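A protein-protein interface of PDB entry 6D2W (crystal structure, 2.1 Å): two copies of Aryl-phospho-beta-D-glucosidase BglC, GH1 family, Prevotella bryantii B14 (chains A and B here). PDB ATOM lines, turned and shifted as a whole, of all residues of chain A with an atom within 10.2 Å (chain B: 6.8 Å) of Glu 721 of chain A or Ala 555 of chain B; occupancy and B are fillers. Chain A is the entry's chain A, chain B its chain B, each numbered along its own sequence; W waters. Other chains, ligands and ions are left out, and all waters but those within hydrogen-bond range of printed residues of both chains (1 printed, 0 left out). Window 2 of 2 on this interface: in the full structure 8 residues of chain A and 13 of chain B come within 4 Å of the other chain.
No position is printed for both chains.
Water W1 lies within hydrogen-bond range of OD2 of Asp 728 of chain A (2.7 Å) and NZ of Lys 557 of chain B (3.4 Å).
Ala 720 of chain A touches Ala 555 of chain B.
Glu 721 of chain A touches Ala 554 of chain B.
Glu 721 of chain A touches Ala 555 of chain B (OE1 to CB, 3.4 Å).
Ala 554 of chain B touches Lys 724 of chain A.
CE of Lys 724 of chain A touches CD of Lys 557 of chain B (3.9 Å).
CG2 of Thr 765 of chain A touches CG of Glu 558 of chain B, 3.8 Å away.
Printed residues of chain B within 4 Å of Ala 720 of chain A: Ala 555 (3.3 Å).
Glu 721 of chain A touches two residues of chain B.
Printed residues of chain B within 4 Å of Lys 724 of chain A: Ala 554 (3.6 Å) and Lys 557 (3.9 Å).
Ala 727 of chain A touches none of the printed residues of chain B.
Ala 554 of chain B touches just these residues of chain A: Glu 721 and Lys 724.
Ala 555 of chain B touches just these residues of chain A: Ala 720 and Glu 721.
Thr 556 of chain B touches none of the printed residues of chain A.
Of the printed residues of chain A, Lys 557 of chain B touches Lys 724 (3.9 Å).
Printed residues of chain A within 4 Å of Glu 558 of chain B: Thr 765 (3.8 Å).
The nearest residue of chain A that does not touch Ala 555 of chain B is Lys 724 of chain A (5.5 Å).
OD1 of Asp 728 of chain A is in salt-bridge range of NZ of Lys 724 of chain A (2.8 Å).
Printed residues of chain B that touch a printed residue of chain A: Ala 554, Ala 555, Lys 557 and Glu 558.
Hydrophobic or aromatic side chains of chain B that line the printed part of chain A: Ala 554 and Ala 555.
Of the 25 printed residues of chain A, 4 touch a printed residue of chain B.
Printed residues of chain A that touch a printed residue of chain B: Ala 720, Glu 721, Lys 724 and Thr 765.
Hydrophobic or aromatic side chains of chain A within 4 Å of the printed part of chain B: Ala 720.
Among the printed residues, no Asp or Glu carboxylate lies within 4 Å of a Lys or Arg side-chain nitrogen of the other chain.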
ATOM      1  N   PHE A 668      34.762   5.593  21.158  1.00  0.00           N
ATOM      2  CA  PHE A 668      34.443   4.450  20.300  1.00  0.00           C
ATOM      3  C   PHE A 668      32.986   4.462  19.840  1.00  0.00           C
ATOM      4  O   PHE A 668      32.682   3.999  18.735  1.00  0.00           O
ATOM      5  CB  PHE A 668      34.741   3.133  21.029  1.00  0.00           C
ATOM      6  CG  PHE A 668      33.731   2.782  22.098  1.00  0.00           C
ATOM      7  CD1 PHE A 668      32.664   1.930  21.818  1.00  0.00           C
ATOM      8  CD2 PHE A 668      33.848   3.299  23.377  1.00  0.00           C
ATOM      9  CE1 PHE A 668      31.733   1.605  22.789  1.00  0.00           C
ATOM     10  CE2 PHE A 668      32.917   2.976  24.364  1.00  0.00           C
ATOM     11  CZ  PHE A 668      31.860   2.128  24.071  1.00  0.00           C
ATOM     12  N   PHE A 669      32.073   4.966  20.672  1.00  0.00           N
ATOM     13  CA  PHE A 669      30.661   4.937  20.305  1.00  0.00           C
ATOM     14  C   PHE A 669      30.387   5.784  19.068  1.00  0.00           C
ATOM     15  O   PHE A 669      29.457   5.489  18.312  1.00  0.00           O
ATOM     16  CB  PHE A 669      29.795   5.400  21.480  1.00  0.00           C
ATOM     17  CG  PHE A 669      28.321   5.182  21.261  1.00  0.00           C
ATOM     18  CD1 PHE A 669      27.785   3.903  21.287  1.00  0.00           C
ATOM     19  CD2 PHE A 669      27.483   6.246  20.988  1.00  0.00           C
ATOM     20  CE1 PHE A 669      26.433   3.694  21.071  1.00  0.00           C
ATOM     21  CE2 PHE A 669      26.126   6.043  20.770  1.00  0.00           C
ATOM     22  CZ  PHE A 669      25.606   4.764  20.809  1.00  0.00           C
ATOM     23  N   LYS A 672      33.211   3.723  16.033  1.00  0.00           N
ATOM     24  CA  LYS A 672      33.195   2.289  15.765  1.00  0.00           C
ATOM     25  C   LYS A 672      31.784   1.787  15.488  1.00  0.00           C
ATOM     26  O   LYS A 672      30.799   2.336  15.991  1.00  0.00           O
ATOM     27  CB  LYS A 672      33.780   1.497  16.934  1.00  0.00           C
ATOM     28  CG  LYS A 672      35.277   1.646  17.073  1.00  0.00           C
ATOM     29  CD  LYS A 672      35.929   0.301  17.264  1.00  0.00           C
ATOM     30  CE  LYS A 672      37.429   0.362  17.020  1.00  0.00           C
ATOM     31  NZ  LYS A 672      37.798   0.007  15.627  1.00  0.00           N
ATOM     32  N   THR A 673      31.700   0.716  14.696  1.00  0.00           N
ATOM     33  CA  THR A 673      30.426   0.084  14.368  1.00  0.00           C
ATOM     34  C   THR A 673      30.178  -1.200  15.144  1.00  0.00           C
ATOM     35  O   THR A 673      29.018  -1.539  15.402  1.00  0.00           O
ATOM     36  CB  THR A 673      30.344  -0.224  12.867  1.00  0.00           C
ATOM     37  OG1 THR A 673      31.368  -1.161  12.508  1.00  0.00           O
ATOM     38  CG2 THR A 673      30.514   1.048  12.044  1.00  0.00           C
ATOM     39  N   THR A 674      31.234  -1.924  15.511  1.00  0.00           N
ATOM     40  CA  THR A 674      31.133  -3.123  16.330  1.00  0.00           C
ATOM     41  C   THR A 674      32.195  -3.077  17.422  1.00  0.00           C
ATOM     42  O   THR A 674      33.213  -2.391  17.300  1.00  0.00           O
ATOM     43  CB  THR A 674      31.310  -4.401  15.497  1.00  0.00           C
ATOM     44  OG1 THR A 674      32.599  -4.388  14.868  1.00  0.00           O
ATOM     45  CG2 THR A 674      30.237  -4.504  14.425  1.00  0.00           C
ATOM     46  N   TRP A 675      31.941  -3.810  18.504  1.00  0.00           N
ATOM     47  CA  TRP A 675      32.932  -4.004  19.559  1.00  0.00           C
ATOM     48  C   TRP A 675      33.883  -5.097  19.091  1.00  0.00           C
ATOM     49  O   TRP A 675      33.599  -6.287  19.240  1.00  0.00           O
ATOM     50  CB  TRP A 675      32.252  -4.377  20.870  1.00  0.00           C
ATOM     51  CG  TRP A 675      33.178  -4.421  22.034  1.00  0.00           C
ATOM     52  CD1 TRP A 675      33.729  -5.533  22.602  1.00  0.00           C
ATOM     53  CD2 TRP A 675      33.675  -3.301  22.772  1.00  0.00           C
ATOM     54  NE1 TRP A 675      34.539  -5.175  23.653  1.00  0.00           N
ATOM     55  CE2 TRP A 675      34.524  -3.810  23.780  1.00  0.00           C
ATOM     56  CE3 TRP A 675      33.487  -1.919  22.680  1.00  0.00           C
ATOM     57  CZ2 TRP A 675      35.182  -2.984  24.690  1.00  0.00           C
ATOM     58  CZ3 TRP A 675      34.134  -1.097  23.589  1.00  0.00           C
ATOM     59  CH2 TRP A 675      34.976  -1.633  24.581  1.00  0.00           C
ATOM     60  N   THR A 706      29.310   4.297  27.178  1.00  0.00           N
ATOM     61  CA  THR A 706      29.549   4.697  25.795  1.00  0.00           C
ATOM     62  C   THR A 706      29.860   6.179  25.648  1.00  0.00           C
ATOM     63  O   THR A 706      30.068   6.645  24.524  1.00  0.00           O
ATOM     64  CB  THR A 706      28.332   4.357  24.926  1.00  0.00           C
ATOM     65  OG1 THR A 706      27.186   5.055  25.426  1.00  0.00           O
ATOM     66  CG2 THR A 706      28.055   2.880  24.970  1.00  0.00           C
ATOM     67  N   VAL A 714      24.823   6.271  24.142  1.00  0.00           N
ATOM     68  CA  VAL A 714      23.690   5.447  23.739  1.00  0.00           C
ATOM     69  C   VAL A 714      22.436   5.878  24.495  1.00  0.00           C
ATOM     70  O   VAL A 714      22.493   6.338  25.642  1.00  0.00           O
ATOM     71  CB  VAL A 714      24.002   3.954  23.975  1.00  0.00           C
ATOM     72  CG1 VAL A 714      23.968   3.618  25.454  1.00  0.00           C
ATOM     73  CG2 VAL A 714      23.041   3.065  23.195  1.00  0.00           C
ATOM     74  N   SER A 715      21.290   5.757  23.834  1.00  0.00           N
ATOM     75  CA  SER A 715      19.998   5.904  24.484  1.00  0.00           C
ATOM     76  C   SER A 715      19.042   4.902  23.854  1.00  0.00           C
ATOM     77  O   SER A 715      19.369   4.236  22.866  1.00  0.00           O
ATOM     78  CB  SER A 715      19.458   7.334  24.362  1.00  0.00           C
ATOM     79  OG  SER A 715      19.102   7.619  23.021  1.00  0.00           O
ATOM     80  N   LYS A 716      17.841   4.805  24.427  1.00  0.00           N
ATOM     81  CA  LYS A 716      16.857   3.866  23.901  1.00  0.00           C
ATOM     82  C   LYS A 716      16.433   4.214  22.481  1.00  0.00           C
ATOM     83  O   LYS A 716      15.866   3.363  21.786  1.00  0.00           O
ATOM     84  CB  LYS A 716      15.633   3.813  24.817  1.00  0.00           C
ATOM     85  CG  LYS A 716      14.758   5.046  24.758  1.00  0.00           C
ATOM     86  CD  LYS A 716      13.440   4.819  25.495  1.00  0.00           C
ATOM     87  CE  LYS A 716      13.675   4.418  26.948  1.00  0.00           C
ATOM     88  NZ  LYS A 716      12.392   4.216  27.684  1.00  0.00           N
ATOM     89  N   SER A 717      16.692   5.437  22.033  1.00  0.00           N
ATOM     90  CA  SER A 717      16.388   5.827  20.668  1.00  0.00           C
ATOM     91  C   SER A 717      17.572   5.652  19.730  1.00  0.00           C
ATOM     92  O   SER A 717      17.461   5.980  18.546  1.00  0.00           O
ATOM     93  CB  SER A 717      15.900   7.279  20.635  1.00  0.00           C
ATOM     94  OG  SER A 717      16.993   8.174  20.705  1.00  0.00           O
ATOM     95  N   SER A 718      18.698   5.144  20.223  1.00  0.00           N
ATOM     96  CA  SER A 718      19.822   4.849  19.351  1.00  0.00           C
ATOM     97  C   SER A 718      19.463   3.715  18.394  1.00  0.00           C
ATOM     98  O   SER A 718      18.622   2.871  18.712  1.00  0.00           O
ATOM     99  CB  SER A 718      21.048   4.446  20.165  1.00  0.00           C
ATOM    100  OG  SER A 718      21.552   5.519  20.939  1.00  0.00           O
ATOM    101  N   PRO A 719      20.097   3.666  17.222  1.00  0.00           N
ATOM    102  CA  PRO A 719      19.916   2.509  16.337  1.00  0.00           C
ATOM    103  C   PRO A 719      20.278   1.209  17.043  1.00  0.00           C
ATOM    104  O   PRO A 719      21.178   1.161  17.885  1.00  0.00           O
ATOM    105  CB  PRO A 719      20.876   2.794  15.175  1.00  0.00           C
ATOM    106  CG  PRO A 719      21.109   4.264  15.217  1.00  0.00           C
ATOM    107  CD  PRO A 719      21.016   4.667  16.655  1.00  0.00           C
ATOM    108  N   ALA A 720      19.573   0.139  16.667  1.00  0.00           N
ATOM    109  CA  ALA A 720      19.759  -1.148  17.331  1.00  0.00           C
ATOM    110  C   ALA A 720      21.204  -1.640  17.251  1.00  0.00           C
ATOM    111  O   ALA A 720      21.683  -2.296  18.184  1.00  0.00           O
ATOM    112  CB  ALA A 720      18.805  -2.184  16.730  1.00  0.00           C
ATOM    113  N   GLU A 721      21.918  -1.341  16.162  1.00  0.00           N
ATOM    114  CA  GLU A 721      23.307  -1.788  16.062  1.00  0.00           C
ATOM    115  C   GLU A 721      24.219  -1.022  17.013  1.00  0.00           C
ATOM    116  O   GLU A 721      25.261  -1.545  17.429  1.00  0.00           O
ATOM    117  CB  GLU A 721      23.807  -1.655  14.624  1.00  0.00           C
ATOM    118  CG  GLU A 721      23.847  -0.227  14.110  1.00  0.00           C
ATOM    119  CD  GLU A 721      22.531   0.220  13.478  1.00  0.00           C
ATOM    120  OE1 GLU A 721      21.476  -0.404  13.743  1.00  0.00           O
ATOM    121  OE2 GLU A 721      22.560   1.201  12.703  1.00  0.00           O
ATOM    122  N   LYS A 722      23.855   0.216  17.358  1.00  0.00           N
ATOM    123  CA  LYS A 722      24.609   0.963  18.359  1.00  0.00           C
ATOM    124  C   LYS A 722      24.299   0.457  19.762  1.00  0.00           C
ATOM    125  O   LYS A 722      25.176   0.445  20.637  1.00  0.00           O
ATOM    126  CB  LYS A 722      24.293   2.456  18.246  1.00  0.00           C
ATOM    127  CG  LYS A 722      24.919   3.133  17.036  1.00  0.00           C
ATOM    128  CD  LYS A 722      26.431   3.217  17.189  1.00  0.00           C
ATOM    129  CE  LYS A 722      27.088   3.814  15.958  1.00  0.00           C
ATOM    130  NZ  LYS A 722      28.579   3.750  16.053  1.00  0.00           N
ATOM    131  N   ILE A 723      23.049   0.056  20.001  1.00  0.00           N
ATOM    132  CA  ILE A 723      22.719  -0.582  21.270  1.00  0.00           C
ATOM    133  C   ILE A 723      23.500  -1.882  21.415  1.00  0.00           C
ATOM    134  O   ILE A 723      24.036  -2.187  22.488  1.00  0.00           O
ATOM    135  CB  ILE A 723      21.198  -0.797  21.378  1.00  0.00           C
ATOM    136  CG1 ILE A 723      20.486   0.559  21.376  1.00  0.00           C
ATOM    137  CG2 ILE A 723      20.847  -1.554  22.648  1.00  0.00           C
ATOM    138  CD1 ILE A 723      18.981   0.458  21.228  1.00  0.00           C
ATOM    139  N   LYS A 724      23.614  -2.649  20.326  1.00  0.00           N
ATOM    140  CA  LYS A 724      24.450  -3.846  20.350  1.00  0.00           C
ATOM    141  C   LYS A 724      25.893  -3.501  20.698  1.00  0.00           C
ATOM    142  O   LYS A 724      26.538  -4.209  21.478  1.00  0.00           O
ATOM    143  CB  LYS A 724      24.383  -4.568  19.003  1.00  0.00           C
ATOM    144  CG  LYS A 724      24.949  -5.975  19.043  1.00  0.00           C
ATOM    145  CD  LYS A 724      24.931  -6.625  17.674  1.00  0.00           C
ATOM    146  CE  LYS A 724      25.764  -7.894  17.660  1.00  0.00           C
ATOM    147  NZ  LYS A 724      27.188  -7.615  18.007  1.00  0.00           N
ATOM    148  N   LEU A 725      26.414  -2.412  20.130  1.00  0.00           N
ATOM    149  CA  LEU A 725      27.759  -1.969  20.479  1.00  0.00           C
ATOM    150  C   LEU A 725      27.889  -1.741  21.982  1.00  0.00           C
ATOM    151  O   LEU A 725      28.872  -2.173  22.603  1.00  0.00           O
ATOM    152  CB  LEU A 725      28.099  -0.700  19.698  1.00  0.00           C
ATOM    153  CG  LEU A 725      29.448  -0.028  19.953  1.00  0.00           C
ATOM    154  CD1 LEU A 725      30.605  -0.987  19.702  1.00  0.00           C
ATOM    155  CD2 LEU A 725      29.584   1.225  19.088  1.00  0.00           C
ATOM    156  N   ALA A 726      26.894  -1.080  22.585  1.00  0.00           N
ATOM    157  CA  ALA A 726      26.920  -0.806  24.020  1.00  0.00           C
ATOM    158  C   ALA A 726      26.794  -2.089  24.829  1.00  0.00           C
ATOM    159  O   ALA A 726      27.435  -2.236  25.877  1.00  0.00           O
ATOM    160  CB  ALA A 726      25.796   0.165  24.390  1.00  0.00           C
ATOM    161  N   ALA A 727      25.958  -3.021  24.362  1.00  0.00           N
ATOM    162  CA  ALA A 727      25.798  -4.294  25.054  1.00  0.00           C
ATOM    163  C   ALA A 727      27.099  -5.084  25.041  1.00  0.00           C
ATOM    164  O   ALA A 727      27.480  -5.685  26.054  1.00  0.00           O
ATOM    165  CB  ALA A 727      24.667  -5.102  24.412  1.00  0.00           C
ATOM    166  N   ASP A 728      27.809  -5.068  23.905  1.00  0.00           N
ATOM    167  CA  ASP A 728      29.052  -5.826  23.785  1.00  0.00           C
ATOM    168  C   ASP A 728      30.163  -5.226  24.641  1.00  0.00           C
ATOM    169  O   ASP A 728      30.953  -5.973  25.232  1.00  0.00           O
ATOM    170  CB  ASP A 728      29.472  -5.922  22.316  1.00  0.00           C
ATOM    171  CG  ASP A 728      28.511  -6.780  21.484  1.00  0.00           C
ATOM    172  OD1 ASP A 728      28.602  -6.785  20.234  1.00  0.00           O
ATOM    173  OD2 ASP A 728      27.651  -7.456  22.087  1.00  0.00           O
ATOM    174  N   GLN A 729      30.230  -3.894  24.746  1.00  0.00           N
ATOM    175  CA  GLN A 729      31.174  -3.277  25.673  1.00  0.00           C
ATOM    176  C   GLN A 729      30.874  -3.685  27.112  1.00  0.00           C
ATOM    177  O   GLN A 729      31.773  -4.089  27.857  1.00  0.00           O
ATOM    178  CB  GLN A 729      31.144  -1.754  25.544  1.00  0.00           C
ATOM    179  CG  GLN A 729      31.975  -1.061  26.618  1.00  0.00           C
ATOM    180  CD  GLN A 729      31.465   0.325  26.976  1.00  0.00           C
ATOM    181  OE1 GLN A 729      30.303   0.654  26.750  1.00  0.00           O
ATOM    182  NE2 GLN A 729      32.343   1.148  27.534  1.00  0.00           N
ATOM    183  N   THR A 765      18.497  -4.874  26.778  1.00  0.00           N
ATOM    184  CA  THR A 765      19.433  -5.813  26.165  1.00  0.00           C
ATOM    185  C   THR A 765      20.850  -5.609  26.680  1.00  0.00           C
ATOM    186  O   THR A 765      21.636  -6.561  26.710  1.00  0.00           O
ATOM    187  CB  THR A 765      19.414  -5.697  24.638  1.00  0.00           C
ATOM    188  OG1 THR A 765      19.958  -4.432  24.238  1.00  0.00           O
ATOM    189  CG2 THR A 765      17.994  -5.858  24.101  1.00  0.00           C
ATOM    190  N   VAL A 766      21.201  -4.380  27.066  1.00  0.00           N
ATOM    191  CA  VAL A 766      22.513  -4.137  27.660  1.00  0.00           C
ATOM    192  C   VAL A 766      22.600  -4.795  29.033  1.00  0.00           C
ATOM    193  O   VAL A 766      23.601  -5.441  29.363  1.00  0.00           O
ATOM    194  CB  VAL A 766      22.797  -2.625  27.736  1.00  0.00           C
ATOM    195  CG1 VAL A 766      24.087  -2.346  28.510  1.00  0.00           C
ATOM    196  CG2 VAL A 766      22.859  -2.018  26.335  1.00  0.00           C
ATOM    197  N   TRP B 545      13.351  -8.530   6.779  1.00  0.00           N
ATOM    198  CA  TRP B 545      14.284  -7.829   7.651  1.00  0.00           C
ATOM    199  C   TRP B 545      15.397  -8.712   8.201  1.00  0.00           C
ATOM    200  O   TRP B 545      16.307  -8.182   8.852  1.00  0.00           O
ATOM    201  CB  TRP B 545      13.535  -7.183   8.830  1.00  0.00           C
ATOM    202  CG  TRP B 545      12.688  -8.157   9.578  1.00  0.00           C
ATOM    203  CD1 TRP B 545      11.451  -8.612   9.217  1.00  0.00           C
ATOM    204  CD2 TRP B 545      13.015  -8.817  10.809  1.00  0.00           C
ATOM    205  NE1 TRP B 545      10.985  -9.506  10.152  1.00  0.00           N
ATOM    206  CE2 TRP B 545      11.927  -9.655  11.134  1.00  0.00           C
ATOM    207  CE3 TRP B 545      14.121  -8.782  11.664  1.00  0.00           C
ATOM    208  CZ2 TRP B 545      11.906 -10.444  12.281  1.00  0.00           C
ATOM    209  CZ3 TRP B 545      14.102  -9.571  12.806  1.00  0.00           C
ATOM    210  CH2 TRP B 545      13.000 -10.389  13.103  1.00  0.00           C
ATOM    211  N   THR B 550      26.413  -8.523   7.561  1.00  0.00           N
ATOM    212  CA  THR B 550      27.008  -8.153   8.845  1.00  0.00           C
ATOM    213  C   THR B 550      26.231  -7.030   9.527  1.00  0.00           C
ATOM    214  O   THR B 550      25.936  -7.105  10.727  1.00  0.00           O
ATOM    215  CB  THR B 550      28.466  -7.738   8.648  1.00  0.00           C
ATOM    216  OG1 THR B 550      29.156  -8.751   7.907  1.00  0.00           O
ATOM    217  CG2 THR B 550      29.150  -7.544   9.997  1.00  0.00           C
ATOM    218  N   ASP B 551      25.903  -5.972   8.779  1.00  0.00           N
ATOM    219  CA  ASP B 551      25.238  -4.818   9.379  1.00  0.00           C
ATOM    220  C   ASP B 551      23.778  -5.118   9.694  1.00  0.00           C
ATOM    221  O   ASP B 551      23.258  -4.673  10.725  1.00  0.00           O
ATOM    222  CB  ASP B 551      25.347  -3.607   8.454  1.00  0.00           C
ATOM    223  CG  ASP B 551      26.759  -3.051   8.373  1.00  0.00           C
ATOM    224  OD1 ASP B 551      27.463  -3.034   9.407  1.00  0.00           O
ATOM    225  OD2 ASP B 551      27.165  -2.629   7.268  1.00  0.00           O
ATOM    226  N   VAL B 552      23.100  -5.859   8.817  1.00  0.00           N
ATOM    227  CA  VAL B 552      21.723  -6.253   9.093  1.00  0.00           C
ATOM    228  C   VAL B 552      21.665  -7.124  10.344  1.00  0.00           C
ATOM    229  O   VAL B 552      20.795  -6.940  11.207  1.00  0.00           O
ATOM    230  CB  VAL B 552      21.117  -6.968   7.871  1.00  0.00           C
ATOM    231  CG1 VAL B 552      19.777  -7.584   8.225  1.00  0.00           C
ATOM    232  CG2 VAL B 552      20.982  -5.995   6.696  1.00  0.00           C
ATOM    233  N   TYR B 553      22.596  -8.076  10.472  1.00  0.00           N
ATOM    234  CA  TYR B 553      22.605  -8.928  11.657  1.00  0.00           C
ATOM    235  C   TYR B 553      22.746  -8.099  12.925  1.00  0.00           C
ATOM    236  O   TYR B 553      22.045  -8.340  13.914  1.00  0.00           O
ATOM    237  CB  TYR B 553      23.728  -9.964  11.573  1.00  0.00           C
ATOM    238  CG  TYR B 553      23.901 -10.746  12.857  1.00  0.00           C
ATOM    239  CD1 TYR B 553      23.017 -11.762  13.201  1.00  0.00           C
ATOM    240  CD2 TYR B 553      24.934 -10.451  13.735  1.00  0.00           C
ATOM    241  CE1 TYR B 553      23.164 -12.473  14.380  1.00  0.00           C
ATOM    242  CE2 TYR B 553      25.089 -11.154  14.917  1.00  0.00           C
ATOM    243  CZ  TYR B 553      24.202 -12.165  15.232  1.00  0.00           C
ATOM    244  OH  TYR B 553      24.360 -12.868  16.404  1.00  0.00           O
ATOM    245  N   ALA B 554      23.636  -7.103  12.907  1.00  0.00           N
ATOM    246  CA  ALA B 554      23.837  -6.270  14.087  1.00  0.00           C
ATOM    247  C   ALA B 554      22.563  -5.513  14.465  1.00  0.00           C
ATOM    248  O   ALA B 554      22.239  -5.378  15.653  1.00  0.00           O
ATOM    249  CB  ALA B 554      24.996  -5.303  13.845  1.00  0.00           C
ATOM    250  N   ALA B 555      21.822  -5.020  13.471  1.00  0.00           N
ATOM    251  CA  ALA B 555      20.606  -4.260  13.741  1.00  0.00           C
ATOM    252  C   ALA B 555      19.401  -5.133  14.074  1.00  0.00           C
ATOM    253  O   ALA B 555      18.391  -4.605  14.544  1.00  0.00           O
ATOM    254  CB  ALA B 555      20.264  -3.367  12.543  1.00  0.00           C
ATOM    255  N   THR B 556      19.470  -6.442  13.849  1.00  0.00           N
ATOM    256  CA  THR B 556      18.306  -7.298  14.025  1.00  0.00           C
ATOM    257  C   THR B 556      18.513  -8.448  14.994  1.00  0.00           C
ATOM    258  O   THR B 556      17.545  -9.166  15.273  1.00  0.00           O
ATOM    259  CB  THR B 556      17.865  -7.886  12.678  1.00  0.00           C
ATOM    260  OG1 THR B 556      18.926  -8.691  12.142  1.00  0.00           O
ATOM    261  CG2 THR B 556      17.514  -6.773  11.706  1.00  0.00           C
ATOM    262  N   LYS B 557      19.733  -8.653  15.504  1.00  0.00           N
ATOM    263  CA  LYS B 557      20.009  -9.800  16.370  1.00  0.00           C
ATOM    264  C   LYS B 557      19.018  -9.887  17.529  1.00  0.00           C
ATOM    265  O   LYS B 557      18.442 -10.949  17.796  1.00  0.00           O
ATOM    266  CB  LYS B 557      21.440  -9.721  16.912  1.00  0.00           C
ATOM    267  CG  LYS B 557      21.751 -10.789  17.950  1.00  0.00           C
ATOM    268  CD  LYS B 557      23.135 -10.613  18.570  1.00  0.00           C
ATOM    269  CE  LYS B 557      23.398 -11.660  19.650  1.00  0.00           C
ATOM    270  NZ  LYS B 557      24.768 -11.537  20.232  1.00  0.00           N
ATOM    271  N   GLU B 558      18.812  -8.776  18.233  1.00  0.00           N
ATOM    272  CA  GLU B 558      17.974  -8.812  19.426  1.00  0.00           C
ATOM    273  C   GLU B 558      16.500  -8.968  19.061  1.00  0.00           C
ATOM    274  O   GLU B 558      15.763  -9.706  19.724  1.00  0.00           O
ATOM    275  CB  GLU B 558      18.216  -7.550  20.252  1.00  0.00           C
ATOM    276  CG  GLU B 558      19.523  -7.580  21.052  1.00  0.00           C
ATOM    277  CD  GLU B 558      19.843  -8.959  21.632  1.00  0.00           C
ATOM    278  OE1 GLU B 558      20.905  -9.531  21.299  1.00  0.00           O
ATOM    279  OE2 GLU B 558      19.028  -9.471  22.434  1.00  0.00           O
ATOM    280  N   LYS B 559      16.056  -8.284  18.005  1.00  0.00           N
ATOM    281  CA  LYS B 559      14.697  -8.478  17.513  1.00  0.00           C
ATOM    282  C   LYS B 559      14.441  -9.940  17.150  1.00  0.00           C
ATOM    283  O   LYS B 559      13.390 -10.499  17.482  1.00  0.00           O
ATOM    284  CB  LYS B 559      14.466  -7.555  16.314  1.00  0.00           C
ATOM    285  CG  LYS B 559      13.053  -7.526  15.759  1.00  0.00           C
ATOM    286  CD  LYS B 559      12.945  -6.428  14.708  1.00  0.00           C
ATOM    287  CE  LYS B 559      11.884  -6.716  13.665  1.00  0.00           C
ATOM    288  NZ  LYS B 559      11.723  -5.559  12.725  1.00  0.00           N
ATOM    289  N   TYR B 608      22.835 -16.070  13.164  1.00  0.00           N
ATOM    290  CA  TYR B 608      21.386 -16.200  13.290  1.00  0.00           C
ATOM    291  C   TYR B 608      20.993 -17.607  13.720  1.00  0.00           C
ATOM    292  O   TYR B 608      20.161 -17.791  14.617  1.00  0.00           O
ATOM    293  CB  TYR B 608      20.719 -15.887  11.951  1.00  0.00           C
ATOM    294  CG  TYR B 608      20.447 -14.438  11.610  1.00  0.00           C
ATOM    295  CD1 TYR B 608      19.555 -13.673  12.354  1.00  0.00           C
ATOM    296  CD2 TYR B 608      21.027 -13.859  10.487  1.00  0.00           C
ATOM    297  CE1 TYR B 608      19.282 -12.351  12.004  1.00  0.00           C
ATOM    298  CE2 TYR B 608      20.754 -12.554  10.131  1.00  0.00           C
ATOM    299  CZ  TYR B 608      19.881 -11.805  10.885  1.00  0.00           C
ATOM    300  OH  TYR B 608      19.624 -10.505  10.515  1.00  0.00           O
HETATM  301  O   HOH W   1      25.195  -8.373  21.317  1.00  0.00           O
